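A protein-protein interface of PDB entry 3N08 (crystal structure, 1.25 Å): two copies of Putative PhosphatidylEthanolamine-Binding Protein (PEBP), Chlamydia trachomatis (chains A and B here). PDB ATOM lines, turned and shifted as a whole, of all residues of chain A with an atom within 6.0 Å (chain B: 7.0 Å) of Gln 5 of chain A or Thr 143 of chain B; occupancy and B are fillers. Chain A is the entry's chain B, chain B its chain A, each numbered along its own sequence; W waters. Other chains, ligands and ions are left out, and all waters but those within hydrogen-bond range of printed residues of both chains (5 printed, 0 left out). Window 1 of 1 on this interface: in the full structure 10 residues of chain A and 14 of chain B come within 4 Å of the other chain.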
ATOM      1  N   SER A   1     -26.535  -7.949   2.902  1.00  0.00           N
ATOM      2  CA  SER A   1     -27.298  -8.736   3.898  1.00  0.00           C
ATOM      3  C   SER A   1     -27.380  -7.927   5.176  1.00  0.00           C
ATOM      4  O   SER A   1     -26.866  -6.797   5.243  1.00  0.00           O
ATOM      5  CB  SER A   1     -26.659 -10.105   4.149  1.00  0.00           C
ATOM      6  OG  SER A   1     -25.686 -10.098   5.197  1.00  0.00           O
ATOM      7  N   ALA A   3     -26.069  -8.852   8.051  1.00  0.00           N
ATOM      8  CA  ALA A   3     -25.015  -9.235   8.981  1.00  0.00           C
ATOM      9  C   ALA A   3     -23.699  -9.262   8.260  1.00  0.00           C
ATOM     10  O   ALA A   3     -23.628  -9.629   7.084  1.00  0.00           O
ATOM     11  CB  ALA A   3     -25.311 -10.611   9.567  1.00  0.00           C
ATOM     12  N   MET A   4     -22.633  -8.924   8.963  1.00  0.00           N
ATOM     13  CA  MET A   4     -21.302  -8.868   8.383  1.00  0.00           C
ATOM     14  C   MET A   4     -20.943 -10.224   7.811  1.00  0.00           C
ATOM     15  O   MET A   4     -21.233 -11.250   8.414  1.00  0.00           O
ATOM     16  CB  MET A   4     -20.274  -8.472   9.447  1.00  0.00           C
ATOM     17  CG  MET A   4     -18.847  -8.317   8.909  1.00  0.00           C
ATOM     18  SD  MET A   4     -17.647  -7.616  10.095  1.00  0.00           S
ATOM     19  CE  MET A   4     -17.547  -8.944  11.286  1.00  0.00           C
ATOM     20  N   GLN A   5     -20.253 -10.216   6.673  1.00  0.00           N
ATOM     21  CA  GLN A   5     -19.825 -11.406   5.973  1.00  0.00           C
ATOM     22  C   GLN A   5     -18.316 -11.423   5.817  1.00  0.00           C
ATOM     23  O   GLN A   5     -17.668 -10.370   5.628  1.00  0.00           O
ATOM     24  CB  GLN A   5     -20.407 -11.409   4.583  1.00  0.00           C
ATOM     25  CG  GLN A   5     -21.897 -11.362   4.541  1.00  0.00           C
ATOM     26  CD  GLN A   5     -22.380 -11.557   3.126  1.00  0.00           C
ATOM     27  OE1 GLN A   5     -22.035 -12.550   2.482  1.00  0.00           O
ATOM     28  NE2 GLN A   5     -23.107 -10.595   2.599  1.00  0.00           N
ATOM     29  N   LEU A   6     -17.766 -12.635   5.832  1.00  0.00           N
ATOM     30  CA  LEU A   6     -16.384 -12.885   5.474  1.00  0.00           C
ATOM     31  C   LEU A   6     -16.411 -14.031   4.490  1.00  0.00           C
ATOM     32  O   LEU A   6     -16.854 -15.143   4.822  1.00  0.00           O
ATOM     33  CB  LEU A   6     -15.573 -13.253   6.698  1.00  0.00           C
ATOM     34  CG  LEU A   6     -14.123 -13.582   6.379  1.00  0.00           C
ATOM     35  CD1 LEU A   6     -13.377 -12.395   5.828  1.00  0.00           C
ATOM     36  CD2 LEU A   6     -13.416 -14.161   7.586  1.00  0.00           C
ATOM     37  N   THR A   7     -15.963 -13.767   3.269  1.00  0.00           N
ATOM     38  CA  THR A   7     -16.002 -14.750   2.195  1.00  0.00           C
ATOM     39  C   THR A   7     -14.680 -14.745   1.448  1.00  0.00           C
ATOM     40  O   THR A   7     -13.839 -13.889   1.679  1.00  0.00           O
ATOM     41  CB  THR A   7     -17.154 -14.492   1.217  1.00  0.00           C
ATOM     42  OG1 THR A   7     -17.024 -13.177   0.659  1.00  0.00           O
ATOM     43  CG2 THR A   7     -18.491 -14.623   1.928  1.00  0.00           C
ATOM     44  N   SER A  33     -12.803 -11.321   1.484  1.00  0.00           N
ATOM     45  CA  SER A  33     -13.692 -10.164   1.337  1.00  0.00           C
ATOM     46  C   SER A  33     -14.513  -9.961   2.583  1.00  0.00           C
ATOM     47  O   SER A  33     -15.094 -10.910   3.134  1.00  0.00           O
ATOM     48  CB  SER A  33     -14.668 -10.364   0.184  1.00  0.00           C
ATOM     49  OG  SER A  33     -13.977 -10.412  -1.054  1.00  0.00           O
ATOM     50  N   PHE A  34     -14.569  -8.723   3.033  1.00  0.00           N
ATOM     51  CA  PHE A  34     -15.381  -8.316   4.158  1.00  0.00           C
ATOM     52  C   PHE A  34     -16.543  -7.511   3.594  1.00  0.00           C
ATOM     53  O   PHE A  34     -16.340  -6.634   2.740  1.00  0.00           O
ATOM     54  CB  PHE A  34     -14.576  -7.422   5.103  1.00  0.00           C
ATOM     55  CG  PHE A  34     -13.347  -8.076   5.671  1.00  0.00           C
ATOM     56  CD1 PHE A  34     -12.175  -8.154   4.929  1.00  0.00           C
ATOM     57  CD2 PHE A  34     -13.352  -8.619   6.944  1.00  0.00           C
ATOM     58  CE1 PHE A  34     -11.032  -8.760   5.460  1.00  0.00           C
ATOM     59  CE2 PHE A  34     -12.216  -9.196   7.480  1.00  0.00           C
ATOM     60  CZ  PHE A  34     -11.062  -9.279   6.737  1.00  0.00           C
ATOM     61  N   SER A  35     -17.761  -7.794   4.010  1.00  0.00           N
ATOM     62  CA  SER A  35     -18.851  -6.953   3.563  1.00  0.00           C
ATOM     63  C   SER A  35     -19.912  -6.864   4.634  1.00  0.00           C
ATOM     64  O   SER A  35     -19.916  -7.615   5.608  1.00  0.00           O
ATOM     65  CB  SER A  35     -19.431  -7.462   2.249  1.00  0.00           C
ATOM     66  OG  SER A  35     -20.036  -8.727   2.436  1.00  0.00           O
ATOM     67  N   ASP A  36     -20.793  -5.901   4.457  1.00  0.00           N
ATOM     68  CA  ASP A  36     -21.861  -5.619   5.408  1.00  0.00           C
ATOM     69  C   ASP A  36     -21.288  -5.317   6.799  1.00  0.00           C
ATOM     70  O   ASP A  36     -21.843  -5.692   7.821  1.00  0.00           O
ATOM     71  CB  ASP A  36     -22.899  -6.759   5.474  1.00  0.00           C
ATOM     72  CG  ASP A  36     -23.541  -7.049   4.140  1.00  0.00           C
ATOM     73  OD1 ASP A  36     -23.679  -6.111   3.334  1.00  0.00           O
ATOM     74  OD2 ASP A  36     -23.948  -8.209   3.913  1.00  0.00           O
ATOM     75  N   VAL A  37     -20.158  -4.628   6.833  1.00  0.00           N
ATOM     76  CA  VAL A  37     -19.554  -4.237   8.096  1.00  0.00           C
ATOM     77  C   VAL A  37     -20.408  -3.125   8.725  1.00  0.00           C
ATOM     78  O   VAL A  37     -20.761  -2.169   8.041  1.00  0.00           O
ATOM     79  CB  VAL A  37     -18.084  -3.737   7.891  1.00  0.00           C
ATOM     80  CG1 VAL A  37     -17.482  -3.266   9.194  1.00  0.00           C
ATOM     81  CG2 VAL A  37     -17.222  -4.820   7.251  1.00  0.00           C
ATOM     82  N   ALA A 114     -13.668 -13.057  11.563  1.00  0.00           N
ATOM     83  CA  ALA A 114     -13.599 -11.616  11.484  1.00  0.00           C
ATOM     84  C   ALA A 114     -14.375 -11.002  12.642  1.00  0.00           C
ATOM     85  O   ALA A 114     -15.442 -11.499  13.046  1.00  0.00           O
ATOM     86  CB  ALA A 114     -14.167 -11.121  10.166  1.00  0.00           C
ATOM     87  N   THR A 143     -19.395 -10.307  14.396  1.00  0.00           N
ATOM     88  CA  THR A 143     -18.417 -11.286  13.993  1.00  0.00           C
ATOM     89  C   THR A 143     -18.901 -11.957  12.715  1.00  0.00           C
ATOM     90  O   THR A 143     -20.083 -11.842  12.350  1.00  0.00           O
ATOM     91  CB  THR A 143     -18.197 -12.306  15.125  1.00  0.00           C
ATOM     92  OG1 THR A 143     -17.024 -13.099  14.892  1.00  0.00           O
ATOM     93  CG2 THR A 143     -19.427 -13.185  15.288  1.00  0.00           C
ATOM     94  N   ALA A 144     -17.973 -12.603  12.028  1.00  0.00           N
ATOM     95  CA  ALA A 144     -18.283 -13.445  10.891  1.00  0.00           C
ATOM     96  C   ALA A 144     -17.265 -14.571  10.814  1.00  0.00           C
ATOM     97  O   ALA A 144     -16.190 -14.496  11.414  1.00  0.00           O
ATOM     98  CB  ALA A 144     -18.304 -12.642   9.612  1.00  0.00           C
ATOM     99  N   ALA B   3     -20.669 -21.053  -4.089  1.00  0.00           N
ATOM    100  CA  ALA B   3     -21.382 -20.214  -3.107  1.00  0.00           C
ATOM    101  C   ALA B   3     -22.868 -20.534  -3.076  1.00  0.00           C
ATOM    102  O   ALA B   3     -23.485 -20.817  -4.093  1.00  0.00           O
ATOM    103  CB  ALA B   3     -21.161 -18.737  -3.423  1.00  0.00           C
ATOM    104  N   MET B   4     -23.431 -20.510  -1.883  1.00  0.00           N
ATOM    105  CA  MET B   4     -24.862 -20.712  -1.703  1.00  0.00           C
ATOM    106  C   MET B   4     -25.633 -19.727  -2.559  1.00  0.00           C
ATOM    107  O   MET B   4     -25.237 -18.568  -2.693  1.00  0.00           O
ATOM    108  CB  MET B   4     -25.213 -20.558  -0.218  1.00  0.00           C
ATOM    109  CG  MET B   4     -26.661 -20.933   0.101  1.00  0.00           C
ATOM    110  SD  MET B   4     -27.118 -20.962   1.896  1.00  0.00           S
ATOM    111  CE  MET B   4     -27.025 -19.179   2.249  1.00  0.00           C
ATOM    112  N   GLN B   5     -26.751 -20.188  -3.123  1.00  0.00           N
ATOM    113  CA  GLN B   5     -27.580 -19.309  -3.939  1.00  0.00           C
ATOM    114  C   GLN B   5     -29.019 -19.409  -3.521  1.00  0.00           C
ATOM    115  O   GLN B   5     -29.473 -20.430  -3.033  1.00  0.00           O
ATOM    116  CB  GLN B   5     -27.501 -19.665  -5.429  1.00  0.00           C
ATOM    117  CG  GLN B   5     -26.106 -19.682  -6.038  1.00  0.00           C
ATOM    118  CD  GLN B   5     -25.513 -18.312  -6.212  1.00  0.00           C
ATOM    119  OE1 GLN B   5     -26.166 -17.392  -6.713  1.00  0.00           O
ATOM    120  NE2 GLN B   5     -24.251 -18.166  -5.815  1.00  0.00           N
ATOM    121  N   PRO B  38     -24.038 -25.064   2.703  1.00  0.00           N
ATOM    122  CA  PRO B  38     -22.901 -25.832   3.217  1.00  0.00           C
ATOM    123  C   PRO B  38     -23.346 -27.030   4.034  1.00  0.00           C
ATOM    124  O   PRO B  38     -24.354 -26.980   4.742  1.00  0.00           O
ATOM    125  CB  PRO B  38     -22.195 -24.847   4.157  1.00  0.00           C
ATOM    126  CG  PRO B  38     -22.545 -23.505   3.611  1.00  0.00           C
ATOM    127  CD  PRO B  38     -23.961 -23.641   3.081  1.00  0.00           C
ATOM    128  N   TYR B 113     -32.887 -12.366   1.774  1.00  0.00           N
ATOM    129  CA  TYR B 113     -31.607 -12.827   2.282  1.00  0.00           C
ATOM    130  C   TYR B 113     -31.772 -14.190   2.925  1.00  0.00           C
ATOM    131  O   TYR B 113     -32.612 -14.369   3.818  1.00  0.00           O
ATOM    132  CB  TYR B 113     -31.089 -11.855   3.342  1.00  0.00           C
ATOM    133  CG  TYR B 113     -30.915 -10.419   2.853  1.00  0.00           C
ATOM    134  CD1 TYR B 113     -30.034 -10.090   1.837  1.00  0.00           C
ATOM    135  CD2 TYR B 113     -31.645  -9.391   3.426  1.00  0.00           C
ATOM    136  CE1 TYR B 113     -29.889  -8.761   1.399  1.00  0.00           C
ATOM    137  CE2 TYR B 113     -31.503  -8.076   2.984  1.00  0.00           C
ATOM    138  CZ  TYR B 113     -30.621  -7.798   1.979  1.00  0.00           C
ATOM    139  OH  TYR B 113     -30.493  -6.490   1.573  1.00  0.00           O
ATOM    140  N   ALA B 114     -30.967 -15.140   2.487  1.00  0.00           N
ATOM    141  CA  ALA B 114     -30.928 -16.467   3.084  1.00  0.00           C
ATOM    142  C   ALA B 114     -29.632 -16.600   3.867  1.00  0.00           C
ATOM    143  O   ALA B 114     -28.553 -16.207   3.399  1.00  0.00           O
ATOM    144  CB  ALA B 114     -30.968 -17.525   2.014  1.00  0.00           C
ATOM    145  N   TYR B 115     -29.730 -17.186   5.053  1.00  0.00           N
ATOM    146  CA  TYR B 115     -28.570 -17.408   5.912  1.00  0.00           C
ATOM    147  C   TYR B 115     -28.554 -18.890   6.318  1.00  0.00           C
ATOM    148  O   TYR B 115     -29.567 -19.422   6.797  1.00  0.00           O
ATOM    149  CB  TYR B 115     -28.633 -16.570   7.173  1.00  0.00           C
ATOM    150  CG  TYR B 115     -28.854 -15.108   6.936  1.00  0.00           C
ATOM    151  CD1 TYR B 115     -27.781 -14.251   6.863  1.00  0.00           C
ATOM    152  CD2 TYR B 115     -30.140 -14.588   6.772  1.00  0.00           C
ATOM    153  CE1 TYR B 115     -27.961 -12.886   6.633  1.00  0.00           C
ATOM    154  CE2 TYR B 115     -30.332 -13.227   6.545  1.00  0.00           C
ATOM    155  CZ  TYR B 115     -29.241 -12.387   6.491  1.00  0.00           C
ATOM    156  OH  TYR B 115     -29.360 -11.016   6.254  1.00  0.00           O
ATOM    157  N   ALA B 116     -27.407 -19.539   6.143  1.00  0.00           N
ATOM    158  CA  ALA B 116     -27.189 -20.860   6.712  1.00  0.00           C
ATOM    159  C   ALA B 116     -26.532 -20.700   8.075  1.00  0.00           C
ATOM    160  O   ALA B 116     -25.546 -19.960   8.193  1.00  0.00           O
ATOM    161  CB  ALA B 116     -26.308 -21.679   5.787  1.00  0.00           C
ATOM    162  N   ILE B 140     -23.598 -17.676  11.659  1.00  0.00           N
ATOM    163  CA  ILE B 140     -23.838 -17.631  10.239  1.00  0.00           C
ATOM    164  C   ILE B 140     -22.640 -18.245   9.528  1.00  0.00           C
ATOM    165  O   ILE B 140     -21.496 -17.834   9.728  1.00  0.00           O
ATOM    166  CB  ILE B 140     -24.070 -16.184   9.735  1.00  0.00           C
ATOM    167  CG1 ILE B 140     -25.303 -15.588  10.419  1.00  0.00           C
ATOM    168  CG2 ILE B 140     -24.268 -16.177   8.248  1.00  0.00           C
ATOM    169  CD1 ILE B 140     -25.397 -14.089  10.252  1.00  0.00           C
ATOM    170  N   ILE B 141     -22.885 -19.204   8.637  1.00  0.00           N
ATOM    171  CA  ILE B 141     -21.805 -19.806   7.854  1.00  0.00           C
ATOM    172  C   ILE B 141     -21.978 -19.609   6.354  1.00  0.00           C
ATOM    173  O   ILE B 141     -21.051 -19.936   5.617  1.00  0.00           O
ATOM    174  CB  ILE B 141     -21.602 -21.325   8.179  1.00  0.00           C
ATOM    175  CG1 ILE B 141     -22.864 -22.138   7.841  1.00  0.00           C
ATOM    176  CG2 ILE B 141     -21.228 -21.518   9.628  1.00  0.00           C
ATOM    177  CD1 ILE B 141     -22.660 -23.656   7.939  1.00  0.00           C
ATOM    178  N   ALA B 142     -23.112 -19.094   5.888  1.00  0.00           N
ATOM    179  CA  ALA B 142     -23.235 -18.662   4.501  1.00  0.00           C
ATOM    180  C   ALA B 142     -24.400 -17.725   4.363  1.00  0.00           C
ATOM    181  O   ALA B 142     -25.349 -17.789   5.136  1.00  0.00           O
ATOM    182  CB  ALA B 142     -23.424 -19.868   3.541  1.00  0.00           C
ATOM    183  N   THR B 143     -24.341 -16.883   3.327  1.00  0.00           N
ATOM    184  CA  THR B 143     -25.381 -15.911   3.017  1.00  0.00           C
ATOM    185  C   THR B 143     -25.609 -15.900   1.518  1.00  0.00           C
ATOM    186  O   THR B 143     -24.658 -15.995   0.746  1.00  0.00           O
ATOM    187  CB  THR B 143     -24.931 -14.496   3.423  1.00  0.00           C
ATOM    188  OG1 THR B 143     -24.397 -14.522   4.760  1.00  0.00           O
ATOM    189  CG2 THR B 143     -26.073 -13.496   3.358  1.00  0.00           C
ATOM    190  N   ALA B 144     -26.860 -15.762   1.124  1.00  0.00           N
ATOM    191  CA  ALA B 144     -27.201 -15.587  -0.284  1.00  0.00           C
ATOM    192  C   ALA B 144     -28.281 -14.544  -0.406  1.00  0.00           C
ATOM    193  O   ALA B 144     -29.064 -14.319   0.524  1.00  0.00           O
ATOM    194  CB  ALA B 144     -27.693 -16.901  -0.924  1.00  0.00           C
ATOM    195  N   GLU B 145     -28.313 -13.872  -1.558  1.00  0.00           N
ATOM    196  CA  GLU B 145     -29.227 -12.759  -1.799  1.00  0.00           C
ATOM    197  C   GLU B 145     -29.965 -12.921  -3.116  1.00  0.00           C
ATOM    198  O   GLU B 145     -29.353 -13.256  -4.131  1.00  0.00           O
ATOM    199  CB  GLU B 145     -28.429 -11.436  -1.810  1.00  0.00           C
ATOM    200  CG  GLU B 145     -29.229 -10.174  -2.098  1.00  0.00           C
ATOM    201  CD  GLU B 145     -28.352  -8.953  -2.253  1.00  0.00           C
ATOM    202  OE1 GLU B 145     -27.655  -8.611  -1.292  1.00  0.00           O
ATOM    203  OE2 GLU B 145     -28.336  -8.340  -3.332  1.00  0.00           O
HETATM  204  O   HOH W   1     -24.455 -12.608   6.718  1.00  0.00           O
HETATM  205  O   HOH W   2     -22.425 -13.910   0.041  1.00  0.00           O
HETATM  206  O   HOH W   3     -27.813  -5.476   2.266  1.00  0.00           O
HETATM  207  O   HOH W   4     -21.682 -14.810   4.054  1.00  0.00           O
HETATM  208  O   HOH W   5     -26.487  -9.775   0.797  1.00  0.00           O
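OD2 of Asp 36 of chain A lies within hydrogen-bond range of NE2 of Gln 5 of chain A.
The backbone carbonyl oxygen of Ala 3 of chain A lies within hydrogen-bond range of the side-chain hydroxyl of Ser 1 of chain A (2.8 Å).
The backbone NH (N) of Ser 1 of chain A lies within hydrogen-bond range of the side-chain carboxylate (OD2) of Asp 36 of chain A (2.8 Å).
N of Gln 5 of chain A lies within hydrogen-bond range of O of Ser 35 of chain A (2.8 Å).
Among the printed residues, pairs that only touch across the chains: Ser 1 of chain A with Thr 143 of chain B, Ser 1 of chain A with Tyr 115 of chain B, Ala 3 of chain A with Ile 140 of chain B, Ser 1 of chain A with Tyr 113 of chain B and Gln 5 of chain A with Thr 143 of chain B.
Of chain B, only Thr 143 (3.6 Å) comes within 4 Å of Gln 5 of chain A.
Thr 143 of chain B touches two residues of chain A.
Of the printed residues of chain B, Ala 3 of chain A touches Ile 140 (3.5 Å).
Of the printed residues of chain A, Ile 140 of chain B touches Ala 3 (3.5 Å).
Of the printed residues of chain A, Tyr 115 of chain B touches Ser 1 (3.5 Å).
Printed residues of chain A within 4 Å of Tyr 113 of chain B: Ser 1 (3.6 Å).
The nearest residue of chain B that does not touch Gln 5 of chain A is Ala 144 of chain B (6.0 Å).
The nearest printed residue of chain A that does not touch Tyr 115 of chain B is Ala 3 of chain A (4.3 Å).
Of the 14 printed residues of chain A, 3 touch a printed residue of chain B.
Printed residues of chain A that touch a printed residue of chain B: Ser 1, Ala 3 and Gln 5.
Hydrophobic or aromatic side chains of chain A within 4 Å of the printed part of chain B: Ala 3.
Printed residues of chain B that touch a printed residue of chain A: Tyr 113, Tyr 115, Ile 140 and Thr 143.
Among the printed residues, 5 pairs touch across the chains.
Among the printed residues, no Asp or Glu carboxylate lies within 4 Å of a Lys or Arg side-chain nitrogen of the other chain.
Gln 5 of chain A touches Thr 143 of chain B, but with the chains exchanged Thr 143 of chain A does not touch Gln 5 of chain B (18.8 Å).
Positions printed for both chains: 3, 4, 5, 114, 143 and 144.
Water W5 lies within hydrogen-bond range of the side-chain carboxylate of Glu 145 of chain B (2.7 Å) and the backbone NH of Ser 1 of chain A (2.8 Å).
Water W1 lies within hydrogen-bond range of OG1 of Thr 143 of chain B (2.7 Å), O of Ala 3 of chain A (3.1 Å) and OG of Ser 1 of chain A (3.2 Å).
Water W4 bridges OE1 of Gln 5 of chain A (2.8 Å) and OG1 of Thr 143 of chain B (2.8 Å).
Water W2 lies within hydrogen-bond range of the side-chain amide oxygen (OE1) of Gln 5 of chain A (2.8 Å) and the backbone carbonyl oxygen (O) of Thr 143 of chain B (3.1 Å).
Water W3 bridges N of Ser 1 of chain A (2.9 Å) and OH of Tyr 113 of chain B (2.9 Å).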
